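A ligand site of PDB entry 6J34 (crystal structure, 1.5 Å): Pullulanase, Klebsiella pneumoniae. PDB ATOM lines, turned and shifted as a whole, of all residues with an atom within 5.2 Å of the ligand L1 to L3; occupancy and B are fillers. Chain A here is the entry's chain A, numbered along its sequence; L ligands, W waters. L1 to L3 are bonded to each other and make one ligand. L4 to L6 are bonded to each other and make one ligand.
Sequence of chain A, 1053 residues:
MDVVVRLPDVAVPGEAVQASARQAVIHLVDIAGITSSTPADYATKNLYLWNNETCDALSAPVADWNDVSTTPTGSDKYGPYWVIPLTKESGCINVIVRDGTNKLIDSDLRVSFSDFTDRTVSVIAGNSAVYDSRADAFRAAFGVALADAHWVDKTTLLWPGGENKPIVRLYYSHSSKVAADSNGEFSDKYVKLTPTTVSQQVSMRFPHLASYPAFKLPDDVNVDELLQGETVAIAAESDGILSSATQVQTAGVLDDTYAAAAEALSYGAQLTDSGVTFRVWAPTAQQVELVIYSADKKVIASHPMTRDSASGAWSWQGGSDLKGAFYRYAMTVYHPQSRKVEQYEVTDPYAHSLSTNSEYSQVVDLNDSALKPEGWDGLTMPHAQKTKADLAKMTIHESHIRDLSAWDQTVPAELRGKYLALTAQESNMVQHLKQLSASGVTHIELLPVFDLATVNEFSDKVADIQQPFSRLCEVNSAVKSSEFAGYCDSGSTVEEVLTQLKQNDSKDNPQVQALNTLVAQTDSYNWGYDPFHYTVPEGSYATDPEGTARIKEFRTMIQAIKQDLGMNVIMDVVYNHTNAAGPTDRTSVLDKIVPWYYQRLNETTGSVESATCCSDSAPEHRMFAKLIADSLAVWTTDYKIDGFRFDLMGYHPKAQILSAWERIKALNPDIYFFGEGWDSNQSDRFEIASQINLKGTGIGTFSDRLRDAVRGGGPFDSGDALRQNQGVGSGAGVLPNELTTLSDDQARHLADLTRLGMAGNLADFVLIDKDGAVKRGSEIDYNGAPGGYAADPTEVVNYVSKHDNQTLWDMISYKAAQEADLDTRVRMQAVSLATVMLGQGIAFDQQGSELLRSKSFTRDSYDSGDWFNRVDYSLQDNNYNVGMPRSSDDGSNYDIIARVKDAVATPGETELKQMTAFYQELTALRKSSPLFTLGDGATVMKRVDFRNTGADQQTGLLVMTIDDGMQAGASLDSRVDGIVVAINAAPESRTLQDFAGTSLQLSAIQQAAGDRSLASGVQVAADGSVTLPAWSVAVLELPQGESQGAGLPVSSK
The side-chain carboxylate (OD2) of Asp 704 lies within hydrogen-bond range of an oxygen (O2) of LIG L1 (2.6 Å). NH1 of Arg 707 lies within hydrogen-bond range of O3 of LIG L1. The side-chain carboxylate of Asp 860 is in hydrogen-bond range of an oxygen (O2) of LG3 L3 (2.8 Å). O of Thr 612 lies within hydrogen-bond range of O5 of LG3 L3 (2.8 Å). The guanidinium group (NH2) of Arg 859 is in hydrogen-bond range of an oxygen (O2) of LG3 L3 (2.9 Å). O2 of LG2 L2 is in hydrogen-bond range of OD1 of Asn 805, at 3.0 Å. An oxygen (O4) of LG2 L2 sits close to the indole nitrogen (NE1) of Trp 678 (3.5 Å). The side-chain carboxylate (OD1) of Asp 860 lies within hydrogen-bond range of an oxygen (O1) of LG5 L5. The side-chain carboxylate (OD2) of Asp 804 is in hydrogen-bond range of an oxygen (O2) of LG4 L4, at 2.6 Å. An oxygen (O3) of LG6 L6 is in hydrogen-bond range of the backbone carbonyl oxygen (O) of Cys 613, 3.2 Å away. The side-chain carboxylate (OE2) of Glu 676 is in hydrogen-bond range of an oxygen (O1) of LG4 L4, 2.9 Å away.
Water W1 lies within hydrogen-bond range of an oxygen (O6) of LIG L1 and the backbone carbonyl oxygen of Asp 679. Water W6 lies within hydrogen-bond range of O1 of LG3 L3 (2.7 Å), OD1 of Asp 804 (2.8 Å), OD1 of Asp 860 (2.9 Å) and N of Asn 805 (3.3 Å). Water W2 lies within hydrogen-bond range of an oxygen (O2) of LIG L1 (2.7 Å) and the side-chain hydroxyl (OH) of Tyr 782 (2.9 Å). Water W4 lies within hydrogen-bond range of an oxygen (O1) of LG6 L6 (2.6 Å) and an oxygen (O3) of LG3 L3 (2.8 Å). Water W3 lies within hydrogen-bond range of the backbone carbonyl oxygen of Ala 611 (2.7 Å), an oxygen (O5) of LG3 L3 (2.9 Å) and the backbone carbonyl oxygen of Thr 612 (3.3 Å). Water W5 lies within hydrogen-bond range of the side-chain hydroxyl (OH) of Tyr 799 (2.8 Å) and an oxygen (O1) of LG2 L2 (3.0 Å).
O5 of LG2 L2 is in hydrogen-bond range of O1 of LG4 L4 (2.6 Å).
OH of Tyr 782 lies within hydrogen-bond range of O of Asp 704, at 3.3 Å. The guanidinium group (NE) of Arg 707 is in salt-bridge range of the side-chain carboxylate (OD1) of Asp 708, at 2.9 Å. The guanidinium group (NH1) of Arg 707 is in hydrogen-bond range of the side-chain hydroxyl (OH) of Tyr 799 (2.9 Å). The backbone carbonyl oxygen of Arg 859 sits close to the backbone NH of Asn 805. OE2 of Glu 676 is in hydrogen-bond range of NE1 of Trp 678, at 3.1 Å. The backbone NH of Leu 648 sits at hydrogen-bond distance from the side-chain carboxylate of Glu 676, at 2.8 Å. The side-chain carboxylate (OD2) of Asp 708 is in hydrogen-bond range of the side-chain hydroxyl (OH) of Tyr 782 (2.7 Å).
Merely in contact with the ligand L1 to L3: Leu 648, Asp 804, Tyr 782, Pro 715, Cys 613 and Glu 676. Hydrophobic or aromatic side chains that line the ligand L1 to L3: Leu 648, Trp 678 and Pro 715. Within 4 Å of the ligand L1 to L3: Thr 612, Cys 613, Leu 648, Glu 676, Trp 678, Asp 704, Arg 707, Pro 715, Tyr 782, Asp 804, Asn 805, Arg 859 and Asp 860.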
ATOM      1  N   ALA A 611       4.334   3.075   5.779  1.00  0.00           N
ATOM      2  CA  ALA A 611       3.810   2.051   6.667  1.00  0.00           C
ATOM      3  C   ALA A 611       3.482   2.603   8.052  1.00  0.00           C
ATOM      4  O   ALA A 611       2.592   2.070   8.738  1.00  0.00           O
ATOM      5  CB  ALA A 611       4.797   0.896   6.773  1.00  0.00           C
ATOM      6  N   THR A 612       4.174   3.652   8.472  1.00  0.00           N
ATOM      7  CA  THR A 612       3.982   4.208   9.764  1.00  0.00           C
ATOM      8  C   THR A 612       2.726   5.007   9.903  1.00  0.00           C
ATOM      9  O   THR A 612       2.264   5.066  10.975  1.00  0.00           O
ATOM     10  CB  THR A 612       5.138   5.101  10.224  1.00  0.00           C
ATOM     11  OG1 THR A 612       5.279   6.149   9.288  1.00  0.00           O
ATOM     12  CG2 THR A 612       6.380   4.286  10.271  1.00  0.00           C
ATOM     13  N   CYS A 613       2.277   5.549   8.774  1.00  0.00           N
ATOM     14  CA  CYS A 613       1.143   6.441   8.568  1.00  0.00           C
ATOM     15  C   CYS A 613       1.506   7.535   7.566  1.00  0.00           C
ATOM     16  O   CYS A 613       0.757   7.919   6.729  1.00  0.00           O
ATOM     17  CB  CYS A 613       0.752   7.177   9.834  1.00  0.00           C
ATOM     18  SG  CYS A 613       1.988   8.330  10.541  1.00  0.00           S
ATOM     19  N   LEU A 648       6.095   3.546  17.585  1.00  0.00           N
ATOM     20  CA  LEU A 648       6.375   2.533  16.563  1.00  0.00           C
ATOM     21  C   LEU A 648       7.846   2.130  16.545  1.00  0.00           C
ATOM     22  O   LEU A 648       8.547   2.185  15.529  1.00  0.00           O
ATOM     23  CB  LEU A 648       5.872   2.968  15.187  1.00  0.00           C
ATOM     24  CG  LEU A 648       4.344   3.153  15.118  1.00  0.00           C
ATOM     25  CD1 LEU A 648       3.915   3.577  13.720  1.00  0.00           C
ATOM     26  CD2 LEU A 648       3.631   1.862  15.548  1.00  0.00           C
ATOM     27  N   GLU A 676       6.464   1.152  21.583  1.00  0.00           N
ATOM     28  CA  GLU A 676       5.610   0.207  20.865  1.00  0.00           C
ATOM     29  C   GLU A 676       6.503  -0.737  20.089  1.00  0.00           C
ATOM     30  O   GLU A 676       7.017  -0.387  19.035  1.00  0.00           O
ATOM     31  CB  GLU A 676       4.713   0.946  19.893  1.00  0.00           C
ATOM     32  CG  GLU A 676       3.692   1.833  20.525  1.00  0.00           C
ATOM     33  CD  GLU A 676       2.966   2.587  19.462  1.00  0.00           C
ATOM     34  OE1 GLU A 676       3.593   3.485  18.853  1.00  0.00           O
ATOM     35  OE2 GLU A 676       1.794   2.244  19.173  1.00  0.00           O
ATOM     36  N   TRP A 678       5.656  -3.430  18.414  1.00  0.00           N
ATOM     37  CA  TRP A 678       4.901  -4.300  17.527  1.00  0.00           C
ATOM     38  C   TRP A 678       5.750  -4.680  16.319  1.00  0.00           C
ATOM     39  O   TRP A 678       6.673  -3.962  15.929  1.00  0.00           O
ATOM     40  CB  TRP A 678       3.630  -3.611  17.020  1.00  0.00           C
ATOM     41  CG  TRP A 678       2.958  -2.674  17.950  1.00  0.00           C
ATOM     42  CD1 TRP A 678       2.670  -1.357  17.699  1.00  0.00           C
ATOM     43  CD2 TRP A 678       2.405  -2.964  19.250  1.00  0.00           C
ATOM     44  NE1 TRP A 678       2.007  -0.799  18.763  1.00  0.00           N
ATOM     45  CE2 TRP A 678       1.829  -1.764  19.722  1.00  0.00           C
ATOM     46  CE3 TRP A 678       2.356  -4.109  20.062  1.00  0.00           C
ATOM     47  CZ2 TRP A 678       1.202  -1.668  20.970  1.00  0.00           C
ATOM     48  CZ3 TRP A 678       1.742  -4.008  21.307  1.00  0.00           C
ATOM     49  CH2 TRP A 678       1.175  -2.796  21.747  1.00  0.00           C
ATOM     50  N   ASP A 679       5.406  -5.805  15.700  1.00  0.00           N
ATOM     51  CA  ASP A 679       6.035  -6.161  14.445  1.00  0.00           C
ATOM     52  C   ASP A 679       5.793  -5.042  13.434  1.00  0.00           C
ATOM     53  O   ASP A 679       4.681  -4.523  13.299  1.00  0.00           O
ATOM     54  CB  ASP A 679       5.461  -7.483  13.925  1.00  0.00           C
ATOM     55  CG  ASP A 679       6.305  -8.100  12.802  1.00  0.00           C
ATOM     56  OD1 ASP A 679       7.214  -7.425  12.275  1.00  0.00           O
ATOM     57  OD2 ASP A 679       6.037  -9.265  12.436  1.00  0.00           O
ATOM     58  N   ASP A 704       0.433  -6.142  24.522  1.00  0.00           N
ATOM     59  CA  ASP A 704      -0.920  -6.281  24.017  1.00  0.00           C
ATOM     60  C   ASP A 704      -1.629  -7.512  24.563  1.00  0.00           C
ATOM     61  O   ASP A 704      -2.828  -7.689  24.293  1.00  0.00           O
ATOM     62  CB  ASP A 704      -0.953  -6.272  22.481  1.00  0.00           C
ATOM     63  CG  ASP A 704       0.184  -7.061  21.828  1.00  0.00           C
ATOM     64  OD1 ASP A 704       1.108  -7.561  22.514  1.00  0.00           O
ATOM     65  OD2 ASP A 704       0.145  -7.151  20.574  1.00  0.00           O
ATOM     66  N   ARG A 707      -3.707  -6.509  27.840  1.00  0.00           N
ATOM     67  CA  ARG A 707      -4.574  -5.484  27.278  1.00  0.00           C
ATOM     68  C   ARG A 707      -5.790  -6.092  26.580  1.00  0.00           C
ATOM     69  O   ARG A 707      -6.945  -5.774  26.921  1.00  0.00           O
ATOM     70  CB  ARG A 707      -3.750  -4.654  26.288  1.00  0.00           C
ATOM     71  CG  ARG A 707      -4.559  -3.565  25.590  1.00  0.00           C
ATOM     72  CD  ARG A 707      -3.810  -3.126  24.350  1.00  0.00           C
ATOM     73  NE  ARG A 707      -4.033  -4.030  23.226  1.00  0.00           N
ATOM     74  CZ  ARG A 707      -3.352  -3.995  22.083  1.00  0.00           C
ATOM     75  NH1 ARG A 707      -2.356  -3.131  21.916  1.00  0.00           N
ATOM     76  NH2 ARG A 707      -3.648  -4.849  21.121  1.00  0.00           N
ATOM     77  N   ASP A 708      -5.555  -6.974  25.611  1.00  0.00           N
ATOM     78  CA  ASP A 708      -6.680  -7.534  24.854  1.00  0.00           C
ATOM     79  C   ASP A 708      -7.463  -8.565  25.658  1.00  0.00           C
ATOM     80  O   ASP A 708      -8.672  -8.710  25.452  1.00  0.00           O
ATOM     81  CB  ASP A 708      -6.199  -8.134  23.546  1.00  0.00           C
ATOM     82  CG  ASP A 708      -5.819  -7.093  22.517  1.00  0.00           C
ATOM     83  OD1 ASP A 708      -6.132  -5.902  22.730  1.00  0.00           O
ATOM     84  OD2 ASP A 708      -5.218  -7.475  21.502  1.00  0.00           O
ATOM     85  N   PRO A 715      -7.730  -4.041  18.563  1.00  0.00           N
ATOM     86  CA  PRO A 715      -7.878  -2.695  18.040  1.00  0.00           C
ATOM     87  C   PRO A 715      -8.589  -2.565  16.710  1.00  0.00           C
ATOM     88  O   PRO A 715      -9.173  -1.530  16.497  1.00  0.00           O
ATOM     89  CB  PRO A 715      -6.431  -2.222  17.856  1.00  0.00           C
ATOM     90  CG  PRO A 715      -5.636  -3.119  18.685  1.00  0.00           C
ATOM     91  CD  PRO A 715      -6.332  -4.413  18.800  1.00  0.00           C
ATOM     92  N   PHE A 716      -8.530  -3.571  15.874  1.00  0.00           N
ATOM     93  CA  PHE A 716      -9.133  -3.521  14.561  1.00  0.00           C
ATOM     94  C   PHE A 716     -10.534  -4.096  14.417  1.00  0.00           C
ATOM     95  O   PHE A 716     -11.021  -4.271  13.338  1.00  0.00           O
ATOM     96  CB  PHE A 716      -8.285  -4.274  13.568  1.00  0.00           C
ATOM     97  CG  PHE A 716      -6.819  -4.069  13.720  1.00  0.00           C
ATOM     98  CD1 PHE A 716      -6.266  -2.810  13.543  1.00  0.00           C
ATOM     99  CD2 PHE A 716      -6.001  -5.130  14.027  1.00  0.00           C
ATOM    100  CE1 PHE A 716      -4.900  -2.620  13.676  1.00  0.00           C
ATOM    101  CE2 PHE A 716      -4.633  -4.960  14.172  1.00  0.00           C
ATOM    102  CZ  PHE A 716      -4.091  -3.702  13.984  1.00  0.00           C
ATOM    103  N   TYR A 782      -0.736 -16.194  22.180  1.00  0.00           N
ATOM    104  CA  TYR A 782      -1.404 -14.912  21.929  1.00  0.00           C
ATOM    105  C   TYR A 782      -1.487 -14.739  20.414  1.00  0.00           C
ATOM    106  O   TYR A 782      -0.529 -14.296  19.778  1.00  0.00           O
ATOM    107  CB  TYR A 782      -0.667 -13.753  22.595  1.00  0.00           C
ATOM    108  CG  TYR A 782      -1.238 -12.407  22.218  1.00  0.00           C
ATOM    109  CD1 TYR A 782      -2.494 -11.994  22.672  1.00  0.00           C
ATOM    110  CD2 TYR A 782      -0.532 -11.536  21.386  1.00  0.00           C
ATOM    111  CE1 TYR A 782      -3.023 -10.760  22.312  1.00  0.00           C
ATOM    112  CE2 TYR A 782      -1.055 -10.317  21.024  1.00  0.00           C
ATOM    113  CZ  TYR A 782      -2.300  -9.927  21.491  1.00  0.00           C
ATOM    114  OH  TYR A 782      -2.817  -8.698  21.110  1.00  0.00           O
ATOM    115  N   TYR A 799      -1.394  -2.316  30.196  1.00  0.00           N
ATOM    116  CA  TYR A 799      -2.402  -1.262  30.117  1.00  0.00           C
ATOM    117  C   TYR A 799      -3.710  -1.831  29.612  1.00  0.00           C
ATOM    118  O   TYR A 799      -3.738  -2.843  28.903  1.00  0.00           O
ATOM    119  CB  TYR A 799      -1.957  -0.113  29.205  1.00  0.00           C
ATOM    120  CG  TYR A 799      -1.800  -0.437  27.729  1.00  0.00           C
ATOM    121  CD1 TYR A 799      -0.851  -1.351  27.282  1.00  0.00           C
ATOM    122  CD2 TYR A 799      -2.545   0.249  26.767  1.00  0.00           C
ATOM    123  CE1 TYR A 799      -0.682  -1.601  25.912  1.00  0.00           C
ATOM    124  CE2 TYR A 799      -2.372   0.018  25.408  1.00  0.00           C
ATOM    125  CZ  TYR A 799      -1.429  -0.901  24.988  1.00  0.00           C
ATOM    126  OH  TYR A 799      -1.259  -1.135  23.644  1.00  0.00           O
ATOM    127  N   ASP A 804      -4.683   5.671  21.934  1.00  0.00           N
ATOM    128  CA  ASP A 804      -5.094   4.932  20.746  1.00  0.00           C
ATOM    129  C   ASP A 804      -6.278   4.030  21.054  1.00  0.00           C
ATOM    130  O   ASP A 804      -6.331   3.388  22.113  1.00  0.00           O
ATOM    131  CB  ASP A 804      -3.963   4.028  20.269  1.00  0.00           C
ATOM    132  CG  ASP A 804      -2.929   4.752  19.470  1.00  0.00           C
ATOM    133  OD1 ASP A 804      -3.291   5.633  18.657  1.00  0.00           O
ATOM    134  OD2 ASP A 804      -1.743   4.424  19.659  1.00  0.00           O
ATOM    135  N   ASN A 805      -7.203   3.946  20.090  1.00  0.00           N
ATOM    136  CA  ASN A 805      -8.357   3.049  20.147  1.00  0.00           C
ATOM    137  C   ASN A 805      -9.341   3.518  21.193  1.00  0.00           C
ATOM    138  O   ASN A 805      -9.159   4.583  21.801  1.00  0.00           O
ATOM    139  CB  ASN A 805      -7.926   1.594  20.331  1.00  0.00           C
ATOM    140  CG  ASN A 805      -6.925   1.172  19.290  1.00  0.00           C
ATOM    141  OD1 ASN A 805      -5.801   0.756  19.596  1.00  0.00           O
ATOM    142  ND2 ASN A 805      -7.316   1.323  18.031  1.00  0.00           N
ATOM    143  N   ARG A 859     -12.883   5.800  17.884  1.00  0.00           N
ATOM    144  CA  ARG A 859     -11.744   4.880  17.990  1.00  0.00           C
ATOM    145  C   ARG A 859     -10.408   5.612  17.891  1.00  0.00           C
ATOM    146  O   ARG A 859      -9.493   5.329  18.669  1.00  0.00           O
ATOM    147  CB  ARG A 859     -11.827   3.774  16.932  1.00  0.00           C
ATOM    148  CG  ARG A 859     -10.690   2.764  17.116  1.00  0.00           C
ATOM    149  CD  ARG A 859     -10.584   1.775  15.962  1.00  0.00           C
ATOM    150  NE  ARG A 859     -10.184   2.435  14.729  1.00  0.00           N
ATOM    151  CZ  ARG A 859      -8.935   2.760  14.426  1.00  0.00           C
ATOM    152  NH1 ARG A 859      -7.948   2.467  15.263  1.00  0.00           N
ATOM    153  NH2 ARG A 859      -8.674   3.379  13.285  1.00  0.00           N
ATOM    154  N   ASP A 860     -10.267   6.535  16.937  1.00  0.00           N
ATOM    155  CA  ASP A 860      -8.973   7.149  16.620  1.00  0.00           C
ATOM    156  C   ASP A 860      -9.193   8.657  16.660  1.00  0.00           C
ATOM    157  O   ASP A 860      -9.549   9.267  15.647  1.00  0.00           O
ATOM    158  CB  ASP A 860      -8.481   6.670  15.251  1.00  0.00           C
ATOM    159  CG  ASP A 860      -7.090   7.187  14.915  1.00  0.00           C
ATOM    160  OD1 ASP A 860      -6.410   7.741  15.811  1.00  0.00           O
ATOM    161  OD2 ASP A 860      -6.671   7.005  13.757  1.00  0.00           O
HETATM  162  C1  LIG L   1      -0.452  -5.648  17.072  1.00  0.00           C
HETATM  163  C2  LIG L   1      -0.881  -4.909  18.316  1.00  0.00           C
HETATM  164  C3  LIG L   1      -1.703  -3.694  17.987  1.00  0.00           C
HETATM  165  C4  LIG L   1      -0.872  -2.825  17.043  1.00  0.00           C
HETATM  166  C5  LIG L   1      -0.519  -3.615  15.824  1.00  0.00           C
HETATM  167  C6  LIG L   1       0.387  -2.837  14.872  1.00  0.00           C
HETATM  168  O1  LIG L   1      -1.532  -6.225  16.404  1.00  0.00           O
HETATM  169  O2  LIG L   1      -1.625  -5.841  19.105  1.00  0.00           O
HETATM  170  O3  LIG L   1      -1.906  -3.017  19.160  1.00  0.00           O
HETATM  171  O4  LIG L   1      -1.624  -1.690  16.700  1.00  0.00           O
HETATM  172  O5  LIG L   1       0.213  -4.764  16.189  1.00  0.00           O
HETATM  173  O6  LIG L   1       0.587  -3.644  13.754  1.00  0.00           O
HETATM  174  C1  LG2 L   2      -1.134  -0.521  17.318  1.00  0.00           C
HETATM  175  C2  LG2 L   2      -2.214   0.350  17.940  1.00  0.00           C
HETATM  176  C3  LG2 L   2      -3.048   0.912  16.837  1.00  0.00           C
HETATM  177  C4  LG2 L   2      -2.140   1.768  15.990  1.00  0.00           C
HETATM  178  C5  LG2 L   2      -1.134   0.803  15.406  1.00  0.00           C
HETATM  179  C6  LG2 L   2      -0.203   1.435  14.364  1.00  0.00           C
HETATM  180  O1  LG2 L   2      -3.049  -0.429  18.783  1.00  0.00           O
HETATM  181  O2  LG2 L   2      -4.010   1.774  17.374  1.00  0.00           O
HETATM  182  O3  LG2 L   2      -2.936   2.320  14.960  1.00  0.00           O
HETATM  183  O4  LG2 L   2      -0.383   0.289  16.462  1.00  0.00           O
HETATM  184  O5  LG2 L   2       0.234   2.651  14.876  1.00  0.00           O
HETATM  185  C1  LG3 L   3      -3.001   3.737  15.032  1.00  0.00           C
HETATM  186  C2  LG3 L   3      -4.394   4.208  14.652  1.00  0.00           C
HETATM  187  C3  LG3 L   3      -4.763   3.837  13.251  1.00  0.00           C
HETATM  188  C4  LG3 L   3      -3.721   4.410  12.320  1.00  0.00           C
HETATM  189  C5  LG3 L   3      -2.355   3.936  12.797  1.00  0.00           C
HETATM  190  C6  LG3 L   3      -1.288   4.565  11.912  1.00  0.00           C
HETATM  191  O1  LG3 L   3      -5.272   3.617  15.595  1.00  0.00           O
HETATM  192  O2  LG3 L   3      -6.021   4.398  12.914  1.00  0.00           O
HETATM  193  O3  LG3 L   3      -3.958   3.918  11.030  1.00  0.00           O
HETATM  194  O4  LG3 L   3      -2.143   4.338  14.108  1.00  0.00           O
HETATM  195  O5  LG3 L   3      -0.020   4.080  12.297  1.00  0.00           O
HETATM  196  C1  LG4 L   4       1.578   5.188  17.197  1.00  0.00           C
HETATM  197  C2  LG4 L   4       0.716   6.216  17.909  1.00  0.00           C
HETATM  198  C3  LG4 L   4      -0.511   6.500  17.058  1.00  0.00           C
HETATM  199  C4  LG4 L   4      -0.025   7.207  15.802  1.00  0.00           C
HETATM  200  C5  LG4 L   4       0.871   6.197  15.124  1.00  0.00           C
HETATM  201  C6  LG4 L   4       1.606   6.868  13.979  1.00  0.00           C
HETATM  202  O1  LG4 L   4       0.934   3.935  17.015  1.00  0.00           O
HETATM  203  O2  LG4 L   4       0.386   5.780  19.225  1.00  0.00           O
HETATM  204  O3  LG4 L   4      -1.332   7.274  17.862  1.00  0.00           O
HETATM  205  O4  LG4 L   4      -1.091   7.441  14.913  1.00  0.00           O
HETATM  206  O5  LG4 L   4       1.902   5.694  15.945  1.00  0.00           O
HETATM  207  O6  LG4 L   4       2.439   7.829  14.525  1.00  0.00           O
HETATM  208  C1  LG5 L   5      -1.686   8.699  15.022  1.00  0.00           C
HETATM  209  C2  LG5 L   5      -3.141   8.582  14.535  1.00  0.00           C
HETATM  210  C3  LG5 L   5      -3.170   8.315  13.071  1.00  0.00           C
HETATM  211  C4  LG5 L   5      -2.471   9.488  12.385  1.00  0.00           C
HETATM  212  C5  LG5 L   5      -1.042   9.470  12.922  1.00  0.00           C
HETATM  213  C6  LG5 L   5      -0.283  10.634  12.308  1.00  0.00           C
HETATM  214  O1  LG5 L   5      -3.775   7.477  15.175  1.00  0.00           O
HETATM  215  O2  LG5 L   5      -4.512   8.258  12.621  1.00  0.00           O
HETATM  216  O3  LG5 L   5      -2.461   9.332  11.004  1.00  0.00           O
HETATM  217  O4  LG5 L   5      -1.071   9.708  14.278  1.00  0.00           O
HETATM  218  O5  LG5 L   5      -0.767  11.845  12.766  1.00  0.00           O
HETATM  219  C1  LG6 L   6      -3.407  10.143  10.308  1.00  0.00           C
HETATM  220  C2  LG6 L   6      -4.028   9.295   9.235  1.00  0.00           C
HETATM  221  C3  LG6 L   6      -3.015   8.988   8.183  1.00  0.00           C
HETATM  222  C4  LG6 L   6      -2.467  10.321   7.738  1.00  0.00           C
HETATM  223  C5  LG6 L   6      -1.868  11.035   8.905  1.00  0.00           C
HETATM  224  C6  LG6 L   6      -1.309  12.352   8.482  1.00  0.00           C
HETATM  225  O1  LG6 L   6      -4.520   8.079   9.745  1.00  0.00           O
HETATM  226  O2  LG6 L   6      -3.621   8.321   7.105  1.00  0.00           O
HETATM  227  O3  LG6 L   6      -1.514  10.131   6.725  1.00  0.00           O
HETATM  228  O4  LG6 L   6      -2.876  11.321   9.806  1.00  0.00           O
HETATM  229  O5  LG6 L   6      -2.360  13.018   7.762  1.00  0.00           O
HETATM  230  O   HOH W   1       2.295  -5.676  13.921  1.00  0.00           O
HETATM  231  O   HOH W   2      -3.060  -8.028  18.310  1.00  0.00           O
HETATM  232  O   HOH W   3       1.386   1.869  11.094  1.00  0.00           O
HETATM  233  O   HOH W   4      -2.941   6.055   9.588  1.00  0.00           O
HETATM  234  O   HOH W   5      -2.208   0.413  21.577  1.00  0.00           O
HETATM  235  O   HOH W   6      -5.826   5.462  17.501  1.00  0.00           O
